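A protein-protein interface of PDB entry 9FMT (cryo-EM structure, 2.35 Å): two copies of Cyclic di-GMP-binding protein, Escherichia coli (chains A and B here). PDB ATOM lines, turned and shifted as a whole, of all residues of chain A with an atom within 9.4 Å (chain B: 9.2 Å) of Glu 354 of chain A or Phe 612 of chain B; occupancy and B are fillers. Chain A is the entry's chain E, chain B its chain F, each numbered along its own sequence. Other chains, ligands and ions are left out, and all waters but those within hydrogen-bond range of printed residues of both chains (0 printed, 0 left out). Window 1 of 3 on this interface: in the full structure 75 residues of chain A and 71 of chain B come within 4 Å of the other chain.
The backbone carbonyl oxygen (O) of Gly 348 of chain A lies close to the backbone carbonyl oxygen (O) of Phe 612 of chain B, 3.1 Å away. O of Asn 410 of chain B sits at hydrogen-bond distance from NE2 of Gln 358 of chain A. The side-chain carboxylate (OE2) of Glu 354 of chain A lies within salt-bridge range of the side-chain amino group (NZ) of Lys 450 of chain B (3.9 Å).
The backbone NH (N) of Thr 352 of chain A sits at hydrogen-bond distance from the side-chain amide oxygen (OE1) of Gln 356 of chain A. OD2 of Asp 489 of chain A is in salt-bridge range of NZ of Lys 351 of chain A. OE2 of Glu 349 of chain A is in hydrogen-bond range of OG1 of Thr 346 of chain A, at 3.1 Å. The guanidinium group of Arg 343 of chain A is in salt-bridge range of the side-chain carboxylate of Glu 349 of chain A, at 3.3 Å. The backbone NH (N) of Gly 348 of chain A lies within hydrogen-bond range of the backbone carbonyl oxygen (O) of Asp 489 of chain A (3.3 Å).
Among the printed residues, merely in contact across the chains: Glu 354 of chain A with Phe 612 of chain B, Thr 352 of chain A with Phe 612 of chain B, Gln 358 of chain A with Gln 411 of chain B, Lys 351 of chain A with Phe 612 of chain B, Glu 349 of chain A with Phe 612 of chain B, Tyr 353 of chain A with Phe 612 of chain B, Glu 355 of chain A with Asn 410 of chain B and Glu 349 of chain A with Gly 614 of chain B.
Printed residues of chain B within 4 Å of Thr 352 of chain A: Phe 612 (3.3 Å). Glu 354 of chain A touches two residues of chain B. Leu 408 of chain B touches none of the printed residues of chain A. Of the printed residues of chain A, Lys 450 of chain B touches Glu 354. Of chain A, only Gly 348, Glu 349, Lys 351, Thr 352, Tyr 353 and Glu 354 come within 4 Å of Phe 612 of chain B. The nearest residue of chain B that does not touch Glu 354 of chain A is Gln 411 of chain B (6.0 Å). The nearest printed residue of chain A that does not touch Gly 614 of chain B is Thr 346 of chain A (4.4 Å).
Of the 17 printed residues of chain A, 8 touch a printed residue of chain B. Of the 17 printed residues of chain B, 5 touch a printed residue of chain A. Hydrophobic or aromatic side chains of chain B within 4 Å of the printed part of chain A: Phe 612. Among the printed residues, 11 pairs touch across the chains. Among the printed residues, Asp or Glu carboxylates within 4 Å of a Lys or Arg side-chain nitrogen of the other chain: Glu 354 of chain A with Lys 450 of chain B.
No position is printed for both chains. Of the 11 pairs that touch across the chains among the printed residues, none has its exchanged pair printed and touching as well.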
ATOM      1  N   ARG A 144      21.829  14.922   7.307  1.00  0.00           N
ATOM      2  CA  ARG A 144      22.582  13.804   6.755  1.00  0.00           C
ATOM      3  C   ARG A 144      24.061  14.158   6.751  1.00  0.00           C
ATOM      4  O   ARG A 144      24.441  15.239   6.289  1.00  0.00           O
ATOM      5  CB  ARG A 144      22.122  13.471   5.333  1.00  0.00           C
ATOM      6  CG  ARG A 144      20.757  12.820   5.244  1.00  0.00           C
ATOM      7  CD  ARG A 144      20.376  12.572   3.794  1.00  0.00           C
ATOM      8  NE  ARG A 144      19.031  12.025   3.660  1.00  0.00           N
ATOM      9  CZ  ARG A 144      18.380  11.913   2.511  1.00  0.00           C
ATOM     10  NH1 ARG A 144      18.921  12.307   1.369  1.00  0.00           N
ATOM     11  NH2 ARG A 144      17.156  11.394   2.506  1.00  0.00           N
ATOM     12  N   ARG A 343      -7.920  -6.508  -1.350  1.00  0.00           N
ATOM     13  CA  ARG A 343      -7.629  -6.163  -2.731  1.00  0.00           C
ATOM     14  C   ARG A 343      -6.127  -6.113  -2.954  1.00  0.00           C
ATOM     15  O   ARG A 343      -5.357  -5.918  -2.008  1.00  0.00           O
ATOM     16  CB  ARG A 343      -8.251  -4.807  -3.097  1.00  0.00           C
ATOM     17  CG  ARG A 343      -7.712  -3.648  -2.281  1.00  0.00           C
ATOM     18  CD  ARG A 343      -8.283  -2.327  -2.754  1.00  0.00           C
ATOM     19  NE  ARG A 343      -7.427  -1.696  -3.750  1.00  0.00           N
ATOM     20  CZ  ARG A 343      -6.449  -0.848  -3.467  1.00  0.00           C
ATOM     21  NH1 ARG A 343      -6.171  -0.507  -2.220  1.00  0.00           N
ATOM     22  NH2 ARG A 343      -5.731  -0.330  -4.459  1.00  0.00           N
ATOM     23  N   VAL A 345      -2.594  -4.544  -3.712  1.00  0.00           N
ATOM     24  CA  VAL A 345      -2.050  -3.259  -3.291  1.00  0.00           C
ATOM     25  C   VAL A 345      -0.846  -2.933  -4.160  1.00  0.00           C
ATOM     26  O   VAL A 345       0.034  -3.779  -4.357  1.00  0.00           O
ATOM     27  CB  VAL A 345      -1.662  -3.270  -1.802  1.00  0.00           C
ATOM     28  CG1 VAL A 345      -2.897  -3.103  -0.936  1.00  0.00           C
ATOM     29  CG2 VAL A 345      -0.947  -4.559  -1.461  1.00  0.00           C
ATOM     30  N   THR A 346      -0.807  -1.709  -4.676  1.00  0.00           N
ATOM     31  CA  THR A 346       0.318  -1.265  -5.479  1.00  0.00           C
ATOM     32  C   THR A 346       1.527  -0.982  -4.593  1.00  0.00           C
ATOM     33  O   THR A 346       1.411  -0.777  -3.381  1.00  0.00           O
ATOM     34  CB  THR A 346      -0.047  -0.015  -6.278  1.00  0.00           C
ATOM     35  OG1 THR A 346      -0.529   0.999  -5.391  1.00  0.00           O
ATOM     36  CG2 THR A 346      -1.122  -0.333  -7.303  1.00  0.00           C
ATOM     37  N   PHE A 347       2.705  -0.975  -5.218  1.00  0.00           N
ATOM     38  CA  PHE A 347       3.930  -0.671  -4.488  1.00  0.00           C
ATOM     39  C   PHE A 347       4.009   0.793  -4.081  1.00  0.00           C
ATOM     40  O   PHE A 347       4.810   1.138  -3.208  1.00  0.00           O
ATOM     41  CB  PHE A 347       5.153  -1.040  -5.325  1.00  0.00           C
ATOM     42  CG  PHE A 347       5.612  -2.456  -5.137  1.00  0.00           C
ATOM     43  CD1 PHE A 347       4.701  -3.478  -4.948  1.00  0.00           C
ATOM     44  CD2 PHE A 347       6.960  -2.765  -5.152  1.00  0.00           C
ATOM     45  CE1 PHE A 347       5.122  -4.779  -4.779  1.00  0.00           C
ATOM     46  CE2 PHE A 347       7.387  -4.065  -4.983  1.00  0.00           C
ATOM     47  CZ  PHE A 347       6.466  -5.073  -4.796  1.00  0.00           C
ATOM     48  N   GLY A 348       3.201   1.660  -4.696  1.00  0.00           N
ATOM     49  CA  GLY A 348       3.172   3.056  -4.302  1.00  0.00           C
ATOM     50  C   GLY A 348       2.517   3.300  -2.962  1.00  0.00           C
ATOM     51  O   GLY A 348       2.781   4.330  -2.333  1.00  0.00           O
ATOM     52  N   GLU A 349       1.668   2.380  -2.511  1.00  0.00           N
ATOM     53  CA  GLU A 349       1.037   2.485  -1.204  1.00  0.00           C
ATOM     54  C   GLU A 349       1.866   1.856  -0.094  1.00  0.00           C
ATOM     55  O   GLU A 349       1.502   1.988   1.078  1.00  0.00           O
ATOM     56  CB  GLU A 349      -0.348   1.831  -1.231  1.00  0.00           C
ATOM     57  CG  GLU A 349      -1.186   2.209  -2.435  1.00  0.00           C
ATOM     58  CD  GLU A 349      -2.449   1.381  -2.544  1.00  0.00           C
ATOM     59  OE1 GLU A 349      -2.846   0.766  -1.533  1.00  0.00           O
ATOM     60  OE2 GLU A 349      -3.045   1.344  -3.641  1.00  0.00           O
ATOM     61  N   LEU A 350       2.961   1.180  -0.430  1.00  0.00           N
ATOM     62  CA  LEU A 350       3.809   0.526   0.556  1.00  0.00           C
ATOM     63  C   LEU A 350       5.110   1.271   0.816  1.00  0.00           C
ATOM     64  O   LEU A 350       5.890   0.840   1.669  1.00  0.00           O
ATOM     65  CB  LEU A 350       4.126  -0.904   0.112  1.00  0.00           C
ATOM     66  CG  LEU A 350       2.946  -1.857  -0.069  1.00  0.00           C
ATOM     67  CD1 LEU A 350       3.371  -3.079  -0.858  1.00  0.00           C
ATOM     68  CD2 LEU A 350       2.375  -2.255   1.277  1.00  0.00           C
ATOM     69  N   LYS A 351       5.366   2.368   0.112  1.00  0.00           N
ATOM     70  CA  LYS A 351       6.608   3.112   0.261  1.00  0.00           C
ATOM     71  C   LYS A 351       6.404   4.258   1.242  1.00  0.00           C
ATOM     72  O   LYS A 351       5.433   5.013   1.134  1.00  0.00           O
ATOM     73  CB  LYS A 351       7.106   3.633  -1.088  1.00  0.00           C
ATOM     74  CG  LYS A 351       6.112   4.467  -1.865  1.00  0.00           C
ATOM     75  CD  LYS A 351       6.825   5.377  -2.845  1.00  0.00           C
ATOM     76  CE  LYS A 351       5.931   5.744  -4.009  1.00  0.00           C
ATOM     77  NZ  LYS A 351       6.594   6.693  -4.940  1.00  0.00           N
ATOM     78  N   THR A 352       7.318   4.371   2.207  1.00  0.00           N
ATOM     79  CA  THR A 352       7.210   5.403   3.228  1.00  0.00           C
ATOM     80  C   THR A 352       7.612   6.776   2.707  1.00  0.00           C
ATOM     81  O   THR A 352       7.050   7.787   3.144  1.00  0.00           O
ATOM     82  CB  THR A 352       8.065   5.035   4.439  1.00  0.00           C
ATOM     83  OG1 THR A 352       9.414   4.800   4.018  1.00  0.00           O
ATOM     84  CG2 THR A 352       7.526   3.781   5.107  1.00  0.00           C
ATOM     85  N   TYR A 353       8.568   6.839   1.785  1.00  0.00           N
ATOM     86  CA  TYR A 353       9.042   8.106   1.252  1.00  0.00           C
ATOM     87  C   TYR A 353       9.182   8.000  -0.258  1.00  0.00           C
ATOM     88  O   TYR A 353       9.353   6.908  -0.806  1.00  0.00           O
ATOM     89  CB  TYR A 353      10.383   8.523   1.876  1.00  0.00           C
ATOM     90  CG  TYR A 353      11.507   7.530   1.670  1.00  0.00           C
ATOM     91  CD1 TYR A 353      11.604   6.387   2.449  1.00  0.00           C
ATOM     92  CD2 TYR A 353      12.476   7.745   0.705  1.00  0.00           C
ATOM     93  CE1 TYR A 353      12.630   5.482   2.262  1.00  0.00           C
ATOM     94  CE2 TYR A 353      13.505   6.849   0.512  1.00  0.00           C
ATOM     95  CZ  TYR A 353      13.578   5.720   1.293  1.00  0.00           C
ATOM     96  OH  TYR A 353      14.603   4.824   1.103  1.00  0.00           O
ATOM     97  N   GLU A 354       9.095   9.145  -0.927  1.00  0.00           N
ATOM     98  CA  GLU A 354       9.304   9.190  -2.365  1.00  0.00           C
ATOM     99  C   GLU A 354      10.755   8.859  -2.691  1.00  0.00           C
ATOM    100  O   GLU A 354      11.654   9.036  -1.864  1.00  0.00           O
ATOM    101  CB  GLU A 354       8.939  10.568  -2.916  1.00  0.00           C
ATOM    102  CG  GLU A 354       8.586  10.574  -4.392  1.00  0.00           C
ATOM    103  CD  GLU A 354       7.514  11.589  -4.730  1.00  0.00           C
ATOM    104  OE1 GLU A 354       7.034  12.278  -3.806  1.00  0.00           O
ATOM    105  OE2 GLU A 354       7.152  11.699  -5.920  1.00  0.00           O
ATOM    106  N   GLU A 355      10.976   8.367  -3.911  1.00  0.00           N
ATOM    107  CA  GLU A 355      12.274   7.896  -4.389  1.00  0.00           C
ATOM    108  C   GLU A 355      12.747   6.646  -3.655  1.00  0.00           C
ATOM    109  O   GLU A 355      13.938   6.322  -3.686  1.00  0.00           O
ATOM    110  CB  GLU A 355      13.351   8.989  -4.301  1.00  0.00           C
ATOM    111  CG  GLU A 355      12.896  10.367  -4.762  1.00  0.00           C
ATOM    112  CD  GLU A 355      12.974  10.540  -6.264  1.00  0.00           C
ATOM    113  OE1 GLU A 355      14.032  10.223  -6.846  1.00  0.00           O
ATOM    114  OE2 GLU A 355      11.975  10.993  -6.864  1.00  0.00           O
ATOM    115  N   GLN A 356      11.836   5.935  -2.990  1.00  0.00           N
ATOM    116  CA  GLN A 356      12.194   4.687  -2.327  1.00  0.00           C
ATOM    117  C   GLN A 356      12.349   3.546  -3.324  1.00  0.00           C
ATOM    118  O   GLN A 356      13.216   2.682  -3.153  1.00  0.00           O
ATOM    119  CB  GLN A 356      11.138   4.332  -1.279  1.00  0.00           C
ATOM    120  CG  GLN A 356      11.311   2.963  -0.648  1.00  0.00           C
ATOM    121  CD  GLN A 356      10.339   2.718   0.484  1.00  0.00           C
ATOM    122  OE1 GLN A 356       9.907   3.651   1.158  1.00  0.00           O
ATOM    123  NE2 GLN A 356       9.989   1.457   0.699  1.00  0.00           N
ATOM    124  N   LEU A 357      11.529   3.534  -4.372  1.00  0.00           N
ATOM    125  CA  LEU A 357      11.502   2.447  -5.338  1.00  0.00           C
ATOM    126  C   LEU A 357      12.478   2.653  -6.488  1.00  0.00           C
ATOM    127  O   LEU A 357      12.305   2.044  -7.550  1.00  0.00           O
ATOM    128  CB  LEU A 357      10.084   2.266  -5.883  1.00  0.00           C
ATOM    129  CG  LEU A 357       9.019   1.818  -4.885  1.00  0.00           C
ATOM    130  CD1 LEU A 357       7.702   1.571  -5.595  1.00  0.00           C
ATOM    131  CD2 LEU A 357       9.471   0.577  -4.148  1.00  0.00           C
ATOM    132  N   GLN A 358      13.494   3.492  -6.307  1.00  0.00           N
ATOM    133  CA  GLN A 358      14.490   3.721  -7.340  1.00  0.00           C
ATOM    134  C   GLN A 358      15.866   3.834  -6.701  1.00  0.00           C
ATOM    135  O   GLN A 358      15.999   4.215  -5.536  1.00  0.00           O
ATOM    136  CB  GLN A 358      14.178   4.980  -8.157  1.00  0.00           C
ATOM    137  CG  GLN A 358      14.417   6.280  -7.424  1.00  0.00           C
ATOM    138  CD  GLN A 358      13.820   7.465  -8.147  1.00  0.00           C
ATOM    139  OE1 GLN A 358      12.671   7.424  -8.582  1.00  0.00           O
ATOM    140  NE2 GLN A 358      14.599   8.527  -8.286  1.00  0.00           N
ATOM    141  N   ASP A 489       5.740   2.036  -9.634  1.00  0.00           N
ATOM    142  CA  ASP A 489       4.712   2.237  -8.622  1.00  0.00           C
ATOM    143  C   ASP A 489       3.475   1.392  -8.881  1.00  0.00           C
ATOM    144  O   ASP A 489       2.730   1.098  -7.941  1.00  0.00           O
ATOM    145  CB  ASP A 489       4.321   3.713  -8.556  1.00  0.00           C
ATOM    146  CG  ASP A 489       5.022   4.454  -7.440  1.00  0.00           C
ATOM    147  OD1 ASP A 489       6.196   4.136  -7.159  1.00  0.00           O
ATOM    148  OD2 ASP A 489       4.400   5.357  -6.845  1.00  0.00           O
ATOM    149  N   LEU B 408      11.823  11.189 -16.407  1.00  0.00           N
ATOM    150  CA  LEU B 408      10.675  12.057 -16.176  1.00  0.00           C
ATOM    151  C   LEU B 408      10.449  12.162 -14.677  1.00  0.00           C
ATOM    152  O   LEU B 408      10.239  11.144 -14.008  1.00  0.00           O
ATOM    153  CB  LEU B 408       9.425  11.519 -16.872  1.00  0.00           C
ATOM    154  CG  LEU B 408       8.171  12.394 -16.848  1.00  0.00           C
ATOM    155  CD1 LEU B 408       8.366  13.639 -17.692  1.00  0.00           C
ATOM    156  CD2 LEU B 408       6.963  11.607 -17.323  1.00  0.00           C
ATOM    157  N   ASN B 409      10.486  13.388 -14.157  1.00  0.00           N
ATOM    158  CA  ASN B 409      10.293  13.655 -12.732  1.00  0.00           C
ATOM    159  C   ASN B 409      11.275  12.850 -11.881  1.00  0.00           C
ATOM    160  O   ASN B 409      10.898  12.199 -10.905  1.00  0.00           O
ATOM    161  CB  ASN B 409       8.847  13.381 -12.316  1.00  0.00           C
ATOM    162  CG  ASN B 409       7.873  14.371 -12.917  1.00  0.00           C
ATOM    163  OD1 ASN B 409       8.147  15.568 -12.977  1.00  0.00           O
ATOM    164  ND2 ASN B 409       6.729  13.874 -13.369  1.00  0.00           N
ATOM    165  N   ASN B 410      12.550  12.904 -12.269  1.00  0.00           N
ATOM    166  CA  ASN B 410      13.633  12.218 -11.561  1.00  0.00           C
ATOM    167  C   ASN B 410      13.381  10.715 -11.465  1.00  0.00           C
ATOM    168  O   ASN B 410      13.661  10.084 -10.445  1.00  0.00           O
ATOM    169  CB  ASN B 410      13.853  12.820 -10.171  1.00  0.00           C
ATOM    170  CG  ASN B 410      15.286  12.699  -9.705  1.00  0.00           C
ATOM    171  OD1 ASN B 410      16.158  12.255 -10.452  1.00  0.00           O
ATOM    172  ND2 ASN B 410      15.540  13.092  -8.463  1.00  0.00           N
ATOM    173  N   GLN B 411      12.849  10.137 -12.538  1.00  0.00           N
ATOM    174  CA  GLN B 411      12.583   8.706 -12.610  1.00  0.00           C
ATOM    175  C   GLN B 411      13.068   8.191 -13.954  1.00  0.00           C
ATOM    176  O   GLN B 411      12.610   8.660 -15.001  1.00  0.00           O
ATOM    177  CB  GLN B 411      11.094   8.411 -12.421  1.00  0.00           C
ATOM    178  CG  GLN B 411      10.799   7.348 -11.380  1.00  0.00           C
ATOM    179  CD  GLN B 411       9.351   7.355 -10.941  1.00  0.00           C
ATOM    180  OE1 GLN B 411       8.786   8.407 -10.644  1.00  0.00           O
ATOM    181  NE2 GLN B 411       8.740   6.177 -10.898  1.00  0.00           N
ATOM    182  N   LYS B 450       1.222   9.073 -13.945  1.00  0.00           N
ATOM    183  CA  LYS B 450       1.598   9.862 -12.778  1.00  0.00           C
ATOM    184  C   LYS B 450       2.020  11.260 -13.203  1.00  0.00           C
ATOM    185  O   LYS B 450       2.986  11.824 -12.679  1.00  0.00           O
ATOM    186  CB  LYS B 450       2.711   9.176 -11.988  1.00  0.00           C
ATOM    187  CG  LYS B 450       2.657   9.413 -10.487  1.00  0.00           C
ATOM    188  CD  LYS B 450       3.811   8.720  -9.777  1.00  0.00           C
ATOM    189  CE  LYS B 450       3.901   9.140  -8.319  1.00  0.00           C
ATOM    190  NZ  LYS B 450       4.219  10.587  -8.174  1.00  0.00           N
ATOM    191  N   ARG B 508      -4.829  19.332  -4.647  1.00  0.00           N
ATOM    192  CA  ARG B 508      -3.529  19.426  -5.301  1.00  0.00           C
ATOM    193  C   ARG B 508      -3.671  19.999  -6.703  1.00  0.00           C
ATOM    194  O   ARG B 508      -2.897  20.876  -7.107  1.00  0.00           O
ATOM    195  CB  ARG B 508      -2.862  18.053  -5.348  1.00  0.00           C
ATOM    196  CG  ARG B 508      -1.525  18.037  -6.063  1.00  0.00           C
ATOM    197  CD  ARG B 508      -0.379  17.969  -5.073  1.00  0.00           C
ATOM    198  NE  ARG B 508      -0.297  16.664  -4.429  1.00  0.00           N
ATOM    199  CZ  ARG B 508       0.279  16.443  -3.255  1.00  0.00           C
ATOM    200  NH1 ARG B 508       0.834  17.423  -2.564  1.00  0.00           N
ATOM    201  NH2 ARG B 508       0.294  15.209  -2.763  1.00  0.00           N
ATOM    202  N   ARG B 608      -8.952   5.901   6.632  1.00  0.00           N
ATOM    203  CA  ARG B 608      -7.529   5.604   6.533  1.00  0.00           C
ATOM    204  C   ARG B 608      -6.896   6.555   5.530  1.00  0.00           C
ATOM    205  O   ARG B 608      -7.391   6.692   4.408  1.00  0.00           O
ATOM    206  CB  ARG B 608      -7.294   4.149   6.114  1.00  0.00           C
ATOM    207  CG  ARG B 608      -5.891   3.863   5.614  1.00  0.00           C
ATOM    208  CD  ARG B 608      -5.885   2.713   4.622  1.00  0.00           C
ATOM    209  NE  ARG B 608      -5.981   1.419   5.286  1.00  0.00           N
ATOM    210  CZ  ARG B 608      -5.048   0.478   5.228  1.00  0.00           C
ATOM    211  NH1 ARG B 608      -3.930   0.655   4.544  1.00  0.00           N
ATOM    212  NH2 ARG B 608      -5.241  -0.667   5.874  1.00  0.00           N
ATOM    213  N   GLN B 609      -5.810   7.206   5.938  1.00  0.00           N
ATOM    214  CA  GLN B 609      -5.104   8.174   5.105  1.00  0.00           C
ATOM    215  C   GLN B 609      -3.668   7.702   4.925  1.00  0.00           C
ATOM    216  O   GLN B 609      -2.888   7.691   5.884  1.00  0.00           O
ATOM    217  CB  GLN B 609      -5.151   9.567   5.728  1.00  0.00           C
ATOM    218  CG  GLN B 609      -4.312  10.600   4.998  1.00  0.00           C
ATOM    219  CD  GLN B 609      -5.096  11.852   4.662  1.00  0.00           C
ATOM    220  OE1 GLN B 609      -6.170  11.784   4.068  1.00  0.00           O
ATOM    221  NE2 GLN B 609      -4.560  13.005   5.043  1.00  0.00           N
ATOM    222  N   THR B 610      -3.320   7.312   3.703  1.00  0.00           N
ATOM    223  CA  THR B 610      -1.969   6.879   3.390  1.00  0.00           C
ATOM    224  C   THR B 610      -1.120   8.061   2.933  1.00  0.00           C
ATOM    225  O   THR B 610      -1.642   9.025   2.364  1.00  0.00           O
ATOM    226  CB  THR B 610      -1.989   5.814   2.297  1.00  0.00           C
ATOM    227  OG1 THR B 610      -2.376   6.412   1.053  1.00  0.00           O
ATOM    228  CG2 THR B 610      -2.972   4.709   2.649  1.00  0.00           C
ATOM    229  N   PRO B 611       0.194   8.020   3.175  1.00  0.00           N
ATOM    230  CA  PRO B 611       1.061   9.111   2.709  1.00  0.00           C
ATOM    231  C   PRO B 611       1.111   9.207   1.193  1.00  0.00           C
ATOM    232  O   PRO B 611       0.943  10.294   0.631  1.00  0.00           O
ATOM    233  CB  PRO B 611       2.432   8.751   3.296  1.00  0.00           C
ATOM    234  CG  PRO B 611       2.353   7.298   3.620  1.00  0.00           C
ATOM    235  CD  PRO B 611       0.930   7.033   3.982  1.00  0.00           C
ATOM    236  N   PHE B 612       1.338   8.082   0.522  1.00  0.00           N
ATOM    237  CA  PHE B 612       1.379   8.035  -0.940  1.00  0.00           C
ATOM    238  C   PHE B 612       0.240   7.168  -1.454  1.00  0.00           C
ATOM    239  O   PHE B 612       0.338   5.928  -1.427  1.00  0.00           O
ATOM    240  CB  PHE B 612       2.722   7.500  -1.431  1.00  0.00           C
ATOM    241  CG  PHE B 612       3.887   8.372  -1.071  1.00  0.00           C
ATOM    242  CD1 PHE B 612       4.569   8.184   0.117  1.00  0.00           C
ATOM    243  CD2 PHE B 612       4.297   9.385  -1.920  1.00  0.00           C
ATOM    244  CE1 PHE B 612       5.638   8.988   0.450  1.00  0.00           C
ATOM    245  CE2 PHE B 612       5.365  10.192  -1.591  1.00  0.00           C
ATOM    246  CZ  PHE B 612       6.036   9.992  -0.404  1.00  0.00           C
ATOM    247  N   PRO B 613      -0.850   7.760  -1.928  1.00  0.00           N
ATOM    248  CA  PRO B 613      -1.952   6.962  -2.466  1.00  0.00           C
ATOM    249  C   PRO B 613      -1.697   6.553  -3.908  1.00  0.00           C
ATOM    250  O   PRO B 613      -0.907   7.160  -4.633  1.00  0.00           O
ATOM    251  CB  PRO B 613      -3.151   7.910  -2.368  1.00  0.00           C
ATOM    252  CG  PRO B 613      -2.553   9.276  -2.485  1.00  0.00           C
ATOM    253  CD  PRO B 613      -1.115   9.206  -2.019  1.00  0.00           C
ATOM    254  N   GLY B 614      -2.393   5.497  -4.317  1.00  0.00           N
ATOM    255  CA  GLY B 614      -2.292   4.996  -5.668  1.00  0.00           C
ATOM    256  C   GLY B 614      -3.213   5.735  -6.618  1.00  0.00           C
ATOM    257  O   GLY B 614      -3.814   6.761  -6.293  1.00  0.00           O
ATOM    258  N   ILE B 615      -3.316   5.192  -7.832  1.00  0.00           N
ATOM    259  CA  ILE B 615      -4.204   5.776  -8.830  1.00  0.00           C
ATOM    260  C   ILE B 615      -5.660   5.591  -8.424  1.00  0.00           C
ATOM    261  O   ILE B 615      -6.492   6.486  -8.611  1.00  0.00           O
ATOM    262  CB  ILE B 615      -3.919   5.172 -10.217  1.00  0.00           C
ATOM    263  CG1 ILE B 615      -2.425   5.245 -10.535  1.00  0.00           C
ATOM    264  CG2 ILE B 615      -4.729   5.886 -11.289  1.00  0.00           C
ATOM    265  CD1 ILE B 615      -1.840   6.635 -10.414  1.00  0.00           C
ATOM    266  N   VAL B 616      -5.991   4.433  -7.867  1.00  0.00           N
ATOM    267  CA  VAL B 616      -7.366   4.169  -7.428  1.00  0.00           C
ATOM    268  C   VAL B 616      -7.693   5.064  -6.238  1.00  0.00           C
ATOM    269  O   VAL B 616      -6.939   5.072  -5.249  1.00  0.00           O
ATOM    270  CB  VAL B 616      -7.534   2.692  -7.068  1.00  0.00           C
ATOM    271  CG1 VAL B 616      -8.936   2.428  -6.540  1.00  0.00           C
ATOM    272  CG2 VAL B 616      -7.233   1.813  -8.273  1.00  0.00           C
ATOM    273  N   PHE B 680      -3.439  19.015  -0.553  1.00  0.00           N
ATOM    274  CA  PHE B 680      -4.025  17.916  -1.306  1.00  0.00           C
ATOM    275  C   PHE B 680      -5.362  17.551  -0.674  1.00  0.00           C
ATOM    276  O   PHE B 680      -5.800  18.166   0.302  1.00  0.00           O
ATOM    277  CB  PHE B 680      -3.078  16.712  -1.365  1.00  0.00           C
ATOM    278  CG  PHE B 680      -2.712  16.152  -0.019  1.00  0.00           C
ATOM    279  CD1 PHE B 680      -3.471  15.151   0.561  1.00  0.00           C
ATOM    280  CD2 PHE B 680      -1.598  16.614   0.658  1.00  0.00           C
ATOM    281  CE1 PHE B 680      -3.134  14.632   1.793  1.00  0.00           C
ATOM    282  CE2 PHE B 680      -1.255  16.098   1.889  1.00  0.00           C
ATOM    283  CZ  PHE B 680      -2.023  15.105   2.458  1.00  0.00           C
ATOM    284  N   ARG B 695      -7.693  13.590   2.944  1.00  0.00           N
ATOM    285  CA  ARG B 695      -8.375  12.999   1.793  1.00  0.00           C
ATOM    286  C   ARG B 695      -9.641  12.330   2.316  1.00  0.00           C
ATOM    287  O   ARG B 695      -9.671  11.125   2.569  1.00  0.00           O
ATOM    288  CB  ARG B 695      -7.468  12.013   1.068  1.00  0.00           C
ATOM    289  CG  ARG B 695      -6.839  12.562  -0.195  1.00  0.00           C
ATOM    290  CD  ARG B 695      -5.891  11.561  -0.826  1.00  0.00           C
ATOM    291  NE  ARG B 695      -4.749  11.279   0.035  1.00  0.00           N
ATOM    292  CZ  ARG B 695      -3.510  11.677  -0.213  1.00  0.00           C
ATOM    293  NH1 ARG B 695      -3.213  12.382  -1.292  1.00  0.00           N
ATOM    294  NH2 ARG B 695      -2.543  11.361   0.643  1.00  0.00           N
